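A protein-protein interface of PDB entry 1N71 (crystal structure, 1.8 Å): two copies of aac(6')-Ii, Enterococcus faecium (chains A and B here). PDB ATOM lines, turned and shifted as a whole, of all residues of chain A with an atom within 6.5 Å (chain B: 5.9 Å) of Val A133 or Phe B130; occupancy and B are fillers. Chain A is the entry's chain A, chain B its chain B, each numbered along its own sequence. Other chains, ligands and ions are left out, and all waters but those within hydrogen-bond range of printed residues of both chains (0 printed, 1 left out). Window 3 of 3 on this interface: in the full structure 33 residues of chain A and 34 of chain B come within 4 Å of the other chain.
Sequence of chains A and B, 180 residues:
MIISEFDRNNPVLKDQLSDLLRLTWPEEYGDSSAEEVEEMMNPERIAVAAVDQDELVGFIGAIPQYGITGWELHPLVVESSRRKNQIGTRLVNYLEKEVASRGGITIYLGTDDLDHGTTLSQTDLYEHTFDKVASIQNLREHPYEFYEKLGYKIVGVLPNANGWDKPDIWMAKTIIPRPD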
ATOM      1  N   LEU A 120      13.807   6.553 -13.808  1.00  0.00           N
ATOM      2  CA  LEU A 120      14.851   5.563 -14.072  1.00  0.00           C
ATOM      3  C   LEU A 120      16.102   6.188 -14.673  1.00  0.00           C
ATOM      4  O   LEU A 120      17.149   5.547 -14.745  1.00  0.00           O
ATOM      5  CB  LEU A 120      14.336   4.447 -14.989  1.00  0.00           C
ATOM      6  CG  LEU A 120      13.238   3.536 -14.425  1.00  0.00           C
ATOM      7  CD1 LEU A 120      13.046   2.354 -15.365  1.00  0.00           C
ATOM      8  CD2 LEU A 120      13.626   3.036 -13.035  1.00  0.00           C
ATOM      9  N   LEU A 125      21.559   2.978 -12.017  1.00  0.00           N
ATOM     10  CA  LEU A 125      20.660   1.834 -12.100  1.00  0.00           C
ATOM     11  C   LEU A 125      21.187   0.508 -11.578  1.00  0.00           C
ATOM     12  O   LEU A 125      20.431  -0.459 -11.490  1.00  0.00           O
ATOM     13  CB  LEU A 125      20.158   1.662 -13.536  1.00  0.00           C
ATOM     14  CG  LEU A 125      19.041   2.640 -13.900  1.00  0.00           C
ATOM     15  CD1 LEU A 125      18.602   2.411 -15.341  1.00  0.00           C
ATOM     16  CD2 LEU A 125      17.859   2.439 -12.948  1.00  0.00           C
ATOM     17  N   HIS A 128      19.912  -0.765  -6.361  1.00  0.00           N
ATOM     18  CA  HIS A 128      18.481  -0.943  -6.123  1.00  0.00           C
ATOM     19  C   HIS A 128      17.750  -0.986  -7.463  1.00  0.00           C
ATOM     20  O   HIS A 128      16.655  -0.444  -7.620  1.00  0.00           O
ATOM     21  CB  HIS A 128      17.933   0.205  -5.270  1.00  0.00           C
ATOM     22  CG  HIS A 128      18.642   0.380  -3.962  1.00  0.00           C
ATOM     23  ND1 HIS A 128      18.702  -0.613  -3.008  1.00  0.00           N
ATOM     24  CD2 HIS A 128      19.319   1.435  -3.448  1.00  0.00           C
ATOM     25  CE1 HIS A 128      19.386  -0.180  -1.964  1.00  0.00           C
ATOM     26  NE2 HIS A 128      19.770   1.061  -2.205  1.00  0.00           N
ATOM     27  N   THR A 129      18.389  -1.642  -8.422  1.00  0.00           N
ATOM     28  CA  THR A 129      17.875  -1.792  -9.774  1.00  0.00           C
ATOM     29  C   THR A 129      16.373  -2.041  -9.859  1.00  0.00           C
ATOM     30  O   THR A 129      15.623  -1.216 -10.378  1.00  0.00           O
ATOM     31  CB  THR A 129      18.596  -2.952 -10.490  1.00  0.00           C
ATOM     32  OG1 THR A 129      20.012  -2.759 -10.395  1.00  0.00           O
ATOM     33  CG2 THR A 129      18.197  -3.010 -11.957  1.00  0.00           C
ATOM     34  N   PHE A 130      15.929  -3.176  -9.337  1.00  0.00           N
ATOM     35  CA  PHE A 130      14.523  -3.519  -9.427  1.00  0.00           C
ATOM     36  C   PHE A 130      13.558  -2.774  -8.509  1.00  0.00           C
ATOM     37  O   PHE A 130      12.360  -2.696  -8.805  1.00  0.00           O
ATOM     38  CB  PHE A 130      14.385  -5.039  -9.317  1.00  0.00           C
ATOM     39  CG  PHE A 130      15.087  -5.771 -10.436  1.00  0.00           C
ATOM     40  CD1 PHE A 130      14.674  -5.601 -11.756  1.00  0.00           C
ATOM     41  CD2 PHE A 130      16.200  -6.562 -10.183  1.00  0.00           C
ATOM     42  CE1 PHE A 130      15.362  -6.205 -12.814  1.00  0.00           C
ATOM     43  CE2 PHE A 130      16.899  -7.171 -11.229  1.00  0.00           C
ATOM     44  CZ  PHE A 130      16.480  -6.991 -12.549  1.00  0.00           C
ATOM     45  N   ASP A 131      14.054  -2.214  -7.409  1.00  0.00           N
ATOM     46  CA  ASP A 131      13.176  -1.438  -6.542  1.00  0.00           C
ATOM     47  C   ASP A 131      12.851  -0.158  -7.303  1.00  0.00           C
ATOM     48  O   ASP A 131      11.728   0.345  -7.243  1.00  0.00           O
ATOM     49  CB  ASP A 131      13.851  -1.089  -5.216  1.00  0.00           C
ATOM     50  CG  ASP A 131      13.038  -0.094  -4.393  1.00  0.00           C
ATOM     51  OD1 ASP A 131      13.273   1.125  -4.521  1.00  0.00           O
ATOM     52  OD2 ASP A 131      12.151  -0.529  -3.629  1.00  0.00           O
ATOM     53  N   LYS A 132      13.837   0.357  -8.033  1.00  0.00           N
ATOM     54  CA  LYS A 132      13.633   1.563  -8.825  1.00  0.00           C
ATOM     55  C   LYS A 132      12.659   1.272  -9.971  1.00  0.00           C
ATOM     56  O   LYS A 132      11.779   2.079 -10.264  1.00  0.00           O
ATOM     57  CB  LYS A 132      14.971   2.074  -9.362  1.00  0.00           C
ATOM     58  CG  LYS A 132      15.838   2.700  -8.272  1.00  0.00           C
ATOM     59  CD  LYS A 132      17.265   2.974  -8.730  1.00  0.00           C
ATOM     60  CE  LYS A 132      18.069   3.615  -7.594  1.00  0.00           C
ATOM     61  NZ  LYS A 132      19.494   3.860  -7.951  1.00  0.00           N
ATOM     62  N   VAL A 133      12.805   0.109 -10.598  1.00  0.00           N
ATOM     63  CA  VAL A 133      11.911  -0.276 -11.685  1.00  0.00           C
ATOM     64  C   VAL A 133      10.479  -0.358 -11.163  1.00  0.00           C
ATOM     65  O   VAL A 133       9.556   0.177 -11.774  1.00  0.00           O
ATOM     66  CB  VAL A 133      12.296  -1.653 -12.280  1.00  0.00           C
ATOM     67  CG1 VAL A 133      11.205  -2.137 -13.228  1.00  0.00           C
ATOM     68  CG2 VAL A 133      13.615  -1.545 -13.027  1.00  0.00           C
ATOM     69  N   ALA A 134      10.299  -1.020 -10.025  1.00  0.00           N
ATOM     70  CA  ALA A 134       8.969  -1.173  -9.442  1.00  0.00           C
ATOM     71  C   ALA A 134       8.347   0.161  -9.008  1.00  0.00           C
ATOM     72  O   ALA A 134       7.129   0.335  -9.067  1.00  0.00           O
ATOM     73  CB  ALA A 134       9.034  -2.141  -8.245  1.00  0.00           C
ATOM     74  N   SER A 135       9.176   1.108  -8.585  1.00  0.00           N
ATOM     75  CA  SER A 135       8.666   2.402  -8.131  1.00  0.00           C
ATOM     76  C   SER A 135       8.763   3.506  -9.183  1.00  0.00           C
ATOM     77  O   SER A 135       8.642   4.692  -8.862  1.00  0.00           O
ATOM     78  CB  SER A 135       9.416   2.839  -6.870  1.00  0.00           C
ATOM     79  OG  SER A 135      10.798   3.000  -7.134  1.00  0.00           O
ATOM     80  N   ILE A 136       8.971   3.129 -10.439  1.00  0.00           N
ATOM     81  CA  ILE A 136       9.096   4.131 -11.496  1.00  0.00           C
ATOM     82  C   ILE A 136       7.932   5.116 -11.489  1.00  0.00           C
ATOM     83  O   ILE A 136       6.793   4.746 -11.206  1.00  0.00           O
ATOM     84  CB  ILE A 136       9.171   3.471 -12.898  1.00  0.00           C
ATOM     85  CG1 ILE A 136       9.484   4.532 -13.957  1.00  0.00           C
ATOM     86  CG2 ILE A 136       7.837   2.803 -13.237  1.00  0.00           C
ATOM     87  CD1 ILE A 136       9.753   3.958 -15.339  1.00  0.00           C
ATOM     88  N   GLN A 137       8.236   6.376 -11.789  1.00  0.00           N
ATOM     89  CA  GLN A 137       7.225   7.428 -11.859  1.00  0.00           C
ATOM     90  C   GLN A 137       7.423   8.140 -13.194  1.00  0.00           C
ATOM     91  O   GLN A 137       8.554   8.352 -13.626  1.00  0.00           O
ATOM     92  CB  GLN A 137       7.390   8.431 -10.708  1.00  0.00           C
ATOM     93  CG  GLN A 137       7.199   7.848  -9.320  1.00  0.00           C
ATOM     94  CD  GLN A 137       5.769   7.426  -9.050  1.00  0.00           C
ATOM     95  OE1 GLN A 137       4.833   8.193  -9.265  1.00  0.00           O
ATOM     96  NE2 GLN A 137       5.594   6.203  -8.563  1.00  0.00           N
ATOM     97  N   GLU A 148       2.455   0.370 -20.671  1.00  0.00           N
ATOM     98  CA  GLU A 148       1.919  -0.226 -19.452  1.00  0.00           C
ATOM     99  C   GLU A 148       0.407  -0.349 -19.555  1.00  0.00           C
ATOM    100  O   GLU A 148      -0.165  -1.372 -19.192  1.00  0.00           O
ATOM    101  CB  GLU A 148       2.255   0.616 -18.222  1.00  0.00           C
ATOM    102  CG  GLU A 148       3.716   0.642 -17.856  1.00  0.00           C
ATOM    103  CD  GLU A 148       3.930   0.962 -16.393  1.00  0.00           C
ATOM    104  OE1 GLU A 148       3.233   1.859 -15.870  1.00  0.00           O
ATOM    105  OE2 GLU A 148       4.800   0.322 -15.768  1.00  0.00           O
ATOM    106  N   LYS A 153       4.832  -4.795 -19.337  1.00  0.00           N
ATOM    107  CA  LYS A 153       5.451  -4.595 -18.032  1.00  0.00           C
ATOM    108  C   LYS A 153       6.942  -4.340 -18.189  1.00  0.00           C
ATOM    109  O   LYS A 153       7.572  -4.892 -19.081  1.00  0.00           O
ATOM    110  CB  LYS A 153       5.218  -5.851 -17.183  1.00  0.00           C
ATOM    111  CG  LYS A 153       6.159  -6.049 -16.007  1.00  0.00           C
ATOM    112  CD  LYS A 153       5.832  -7.357 -15.274  1.00  0.00           C
ATOM    113  CE  LYS A 153       6.714  -7.553 -14.050  1.00  0.00           C
ATOM    114  NZ  LYS A 153       6.217  -8.656 -13.170  1.00  0.00           N
ATOM    115  N   ILE A 154       7.510  -3.492 -17.339  1.00  0.00           N
ATOM    116  CA  ILE A 154       8.947  -3.259 -17.418  1.00  0.00           C
ATOM    117  C   ILE A 154       9.585  -4.511 -16.836  1.00  0.00           C
ATOM    118  O   ILE A 154       9.347  -4.855 -15.674  1.00  0.00           O
ATOM    119  CB  ILE A 154       9.392  -2.039 -16.582  1.00  0.00           C
ATOM    120  CG1 ILE A 154       8.732  -0.766 -17.130  1.00  0.00           C
ATOM    121  CG2 ILE A 154      10.930  -1.924 -16.618  1.00  0.00           C
ATOM    122  CD1 ILE A 154       8.983   0.496 -16.287  1.00  0.00           C
ATOM    123  N   VAL A 155      10.387  -5.195 -17.645  1.00  0.00           N
ATOM    124  CA  VAL A 155      11.046  -6.423 -17.218  1.00  0.00           C
ATOM    125  C   VAL A 155      12.560  -6.286 -17.178  1.00  0.00           C
ATOM    126  O   VAL A 155      13.272  -7.252 -16.919  1.00  0.00           O
ATOM    127  CB  VAL A 155      10.706  -7.590 -18.151  1.00  0.00           C
ATOM    128  CG1 VAL A 155       9.224  -7.921 -18.047  1.00  0.00           C
ATOM    129  CG2 VAL A 155      11.074  -7.230 -19.589  1.00  0.00           C
ATOM    130  N   GLY A 156      13.058  -5.089 -17.448  1.00  0.00           N
ATOM    131  CA  GLY A 156      14.494  -4.900 -17.403  1.00  0.00           C
ATOM    132  C   GLY A 156      14.914  -3.506 -17.799  1.00  0.00           C
ATOM    133  O   GLY A 156      14.113  -2.734 -18.328  1.00  0.00           O
ATOM    134  N   VAL A 157      16.175  -3.185 -17.528  1.00  0.00           N
ATOM    135  CA  VAL A 157      16.744  -1.892 -17.873  1.00  0.00           C
ATOM    136  C   VAL A 157      18.186  -2.093 -18.315  1.00  0.00           C
ATOM    137  O   VAL A 157      18.844  -3.046 -17.909  1.00  0.00           O
ATOM    138  CB  VAL A 157      16.744  -0.896 -16.675  1.00  0.00           C
ATOM    139  CG1 VAL A 157      15.312  -0.518 -16.304  1.00  0.00           C
ATOM    140  CG2 VAL A 157      17.480  -1.506 -15.478  1.00  0.00           C
ATOM    141  N   LEU B 125       7.508 -16.671 -15.176  1.00  0.00           N
ATOM    142  CA  LEU B 125       8.315 -15.523 -14.781  1.00  0.00           C
ATOM    143  C   LEU B 125       7.546 -14.231 -14.555  1.00  0.00           C
ATOM    144  O   LEU B 125       8.133 -13.230 -14.145  1.00  0.00           O
ATOM    145  CB  LEU B 125       9.434 -15.267 -15.801  1.00  0.00           C
ATOM    146  CG  LEU B 125      10.817 -15.797 -15.421  1.00  0.00           C
ATOM    147  CD1 LEU B 125      11.873 -15.193 -16.342  1.00  0.00           C
ATOM    148  CD2 LEU B 125      11.125 -15.443 -13.972  1.00  0.00           C
ATOM    149  N   HIS B 128       5.958 -12.875  -9.456  1.00  0.00           N
ATOM    150  CA  HIS B 128       7.112 -12.562  -8.607  1.00  0.00           C
ATOM    151  C   HIS B 128       8.397 -12.494  -9.430  1.00  0.00           C
ATOM    152  O   HIS B 128       9.437 -13.030  -9.040  1.00  0.00           O
ATOM    153  CB  HIS B 128       7.247 -13.624  -7.514  1.00  0.00           C
ATOM    154  CG  HIS B 128       5.950 -13.968  -6.852  1.00  0.00           C
ATOM    155  ND1 HIS B 128       5.189 -13.036  -6.178  1.00  0.00           N
ATOM    156  CD2 HIS B 128       5.260 -15.132  -6.789  1.00  0.00           C
ATOM    157  CE1 HIS B 128       4.086 -13.611  -5.732  1.00  0.00           C
ATOM    158  NE2 HIS B 128       4.105 -14.883  -6.089  1.00  0.00           N
ATOM    159  N   THR B 129       8.317 -11.813 -10.567  1.00  0.00           N
ATOM    160  CA  THR B 129       9.445 -11.682 -11.480  1.00  0.00           C
ATOM    161  C   THR B 129      10.790 -11.341 -10.848  1.00  0.00           C
ATOM    162  O   THR B 129      11.754 -12.105 -10.966  1.00  0.00           O
ATOM    163  CB  THR B 129       9.157 -10.622 -12.556  1.00  0.00           C
ATOM    164  OG1 THR B 129       7.895 -10.903 -13.170  1.00  0.00           O
ATOM    165  CG2 THR B 129      10.245 -10.639 -13.619  1.00  0.00           C
ATOM    166  N   PHE B 130      10.869 -10.192 -10.192  1.00  0.00           N
ATOM    167  CA  PHE B 130      12.129  -9.773  -9.597  1.00  0.00           C
ATOM    168  C   PHE B 130      12.540 -10.554  -8.349  1.00  0.00           C
ATOM    169  O   PHE B 130      13.721 -10.576  -7.993  1.00  0.00           O
ATOM    170  CB  PHE B 130      12.088  -8.268  -9.343  1.00  0.00           C
ATOM    171  CG  PHE B 130      11.742  -7.474 -10.576  1.00  0.00           C
ATOM    172  CD1 PHE B 130      12.295  -7.812 -11.809  1.00  0.00           C
ATOM    173  CD2 PHE B 130      10.838  -6.421 -10.518  1.00  0.00           C
ATOM    174  CE1 PHE B 130      11.951  -7.115 -12.970  1.00  0.00           C
ATOM    175  CE2 PHE B 130      10.486  -5.716 -11.677  1.00  0.00           C
ATOM    176  CZ  PHE B 130      11.043  -6.066 -12.901  1.00  0.00           C
ATOM    177  N   ASP B 131      11.576 -11.189  -7.687  1.00  0.00           N
ATOM    178  CA  ASP B 131      11.883 -12.012  -6.517  1.00  0.00           C
ATOM    179  C   ASP B 131      12.672 -13.220  -7.026  1.00  0.00           C
ATOM    180  O   ASP B 131      13.682 -13.614  -6.436  1.00  0.00           O
ATOM    181  CB  ASP B 131      10.606 -12.517  -5.831  1.00  0.00           C
ATOM    182  CG  ASP B 131       9.897 -11.440  -5.030  1.00  0.00           C
ATOM    183  OD1 ASP B 131      10.567 -10.482  -4.590  1.00  0.00           O
ATOM    184  OD2 ASP B 131       8.667 -11.568  -4.822  1.00  0.00           O
ATOM    185  N   LYS B 132      12.197 -13.801  -8.126  1.00  0.00           N
ATOM    186  CA  LYS B 132      12.848 -14.965  -8.728  1.00  0.00           C
ATOM    187  C   LYS B 132      14.216 -14.609  -9.290  1.00  0.00           C
ATOM    188  O   LYS B 132      15.172 -15.373  -9.140  1.00  0.00           O
ATOM    189  CB  LYS B 132      11.947 -15.566  -9.814  1.00  0.00           C
ATOM    190  CG  LYS B 132      10.709 -16.250  -9.235  1.00  0.00           C
ATOM    191  CD  LYS B 132       9.698 -16.655 -10.296  1.00  0.00           C
ATOM    192  CE  LYS B 132       8.524 -17.383  -9.653  1.00  0.00           C
ATOM    193  NZ  LYS B 132       7.451 -17.745 -10.623  1.00  0.00           N
ATOM    194  N   VAL B 133      14.318 -13.445  -9.929  1.00  0.00           N
ATOM    195  CA  VAL B 133      15.594 -12.996 -10.478  1.00  0.00           C
ATOM    196  C   VAL B 133      16.595 -12.812  -9.340  1.00  0.00           C
ATOM    197  O   VAL B 133      17.770 -13.151  -9.465  1.00  0.00           O
ATOM    198  CB  VAL B 133      15.452 -11.641 -11.221  1.00  0.00           C
ATOM    199  CG1 VAL B 133      16.835 -11.084 -11.556  1.00  0.00           C
ATOM    200  CG2 VAL B 133      14.635 -11.822 -12.501  1.00  0.00           C
ATOM    201  N   ALA B 134      16.116 -12.269  -8.229  1.00  0.00           N
ATOM    202  CA  ALA B 134      16.963 -12.012  -7.067  1.00  0.00           C
ATOM    203  C   ALA B 134      17.479 -13.276  -6.378  1.00  0.00           C
ATOM    204  O   ALA B 134      18.513 -13.243  -5.712  1.00  0.00           O
ATOM    205  CB  ALA B 134      16.201 -11.149  -6.063  1.00  0.00           C
ATOM    206  N   SER B 135      16.767 -14.385  -6.535  1.00  0.00           N
ATOM    207  CA  SER B 135      17.171 -15.634  -5.899  1.00  0.00           C
ATOM    208  C   SER B 135      17.582 -16.704  -6.907  1.00  0.00           C
ATOM    209  O   SER B 135      17.553 -17.904  -6.608  1.00  0.00           O
ATOM    210  CB  SER B 135      16.025 -16.161  -5.032  1.00  0.00           C
ATOM    211  OG  SER B 135      14.909 -16.519  -5.831  1.00  0.00           O
ATOM    212  N   VAL B 157      14.943  -9.691 -17.639  1.00  0.00           N
ATOM    213  CA  VAL B 157      14.598 -11.007 -18.148  1.00  0.00           C
ATOM    214  C   VAL B 157      13.458 -10.859 -19.143  1.00  0.00           C
ATOM    215  O   VAL B 157      12.639  -9.948 -19.030  1.00  0.00           O
ATOM    216  CB  VAL B 157      14.136 -11.964 -17.023  1.00  0.00           C
ATOM    217  CG1 VAL B 157      15.282 -12.241 -16.077  1.00  0.00           C
ATOM    218  CG2 VAL B 157      12.950 -11.355 -16.264  1.00  0.00           C
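The side-chain hydroxyl (OG1) of Thr B129 lies within hydrogen-bond range of the side-chain amino group (NZ) of Lys A153 (2.8 Å).
The backbone carbonyl oxygen of Val A155 sits at hydrogen-bond distance from the backbone NH of Val B157.
The backbone carbonyl oxygen (O) of Leu B125 lies within hydrogen-bond range of the side-chain hydroxyl (OG1) of Thr B129 (2.5 Å).
CD1 of Phe B130 touches CD1 of Phe A130, at 3.2 Å.
Val B133 touches Phe A130 (CG1 to CE2, 3.9 Å).
Phe B130 touches Val A133.
CZ of Phe B130 touches O of Ile A154, at 3.5 Å.
Of chain B, only Phe B130 comes within 4 Å of Val A133.
Phe B130 touches three residues of chain A.
Of the printed residues of chain A, Val B157 touches Val A155.
Printed residues of chain B within 4 Å of Ile A154: Phe B130 (3.5 Å).
Of the printed residues of chain A, Val B133 touches Phe A130 (3.9 Å).
Of the printed residues of chain B, Phe A130 touches Phe B130 (3.2 Å) and Val B133 (3.9 Å).
Of the printed residues of chain A, Thr B129 touches Lys A153.
Glu A148 touches none of the printed residues of chain B.
Asp A131 touches none of the printed residues of chain B.
The nearest printed residue of chain B that does not touch Val A133 is Thr B129 (8.6 Å).
The nearest residue of chain A that does not touch Phe B130 is Val A155 (4.2 Å).
The nearest printed residue of chain A that does not touch Val B157 is Gly A156 (4.8 Å).
Phe A130 touches its own counterpart, Phe B130.
Phe A130 touches Val B133, and with the chains exchanged Val A133 touches Phe B130.
10 positions are printed for both chains.
Of the 6 pairs that touch across the chains among the printed residues, 3 have their exchanged pair printed and touching as well.
Printed residues of chain A that touch a printed residue of chain B: Phe A130, Val A133, Lys A153, Ile A154 and Val A155.
Hydrophobic or aromatic side chains of chain A that line the printed part of chain B: Phe A130, Val A133 and Val A155.
Hydrophobic or aromatic side chains of chain B that line the printed part of chain A: Phe B130 and Val B133.
Among the printed residues, 6 pairs touch across the chains.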
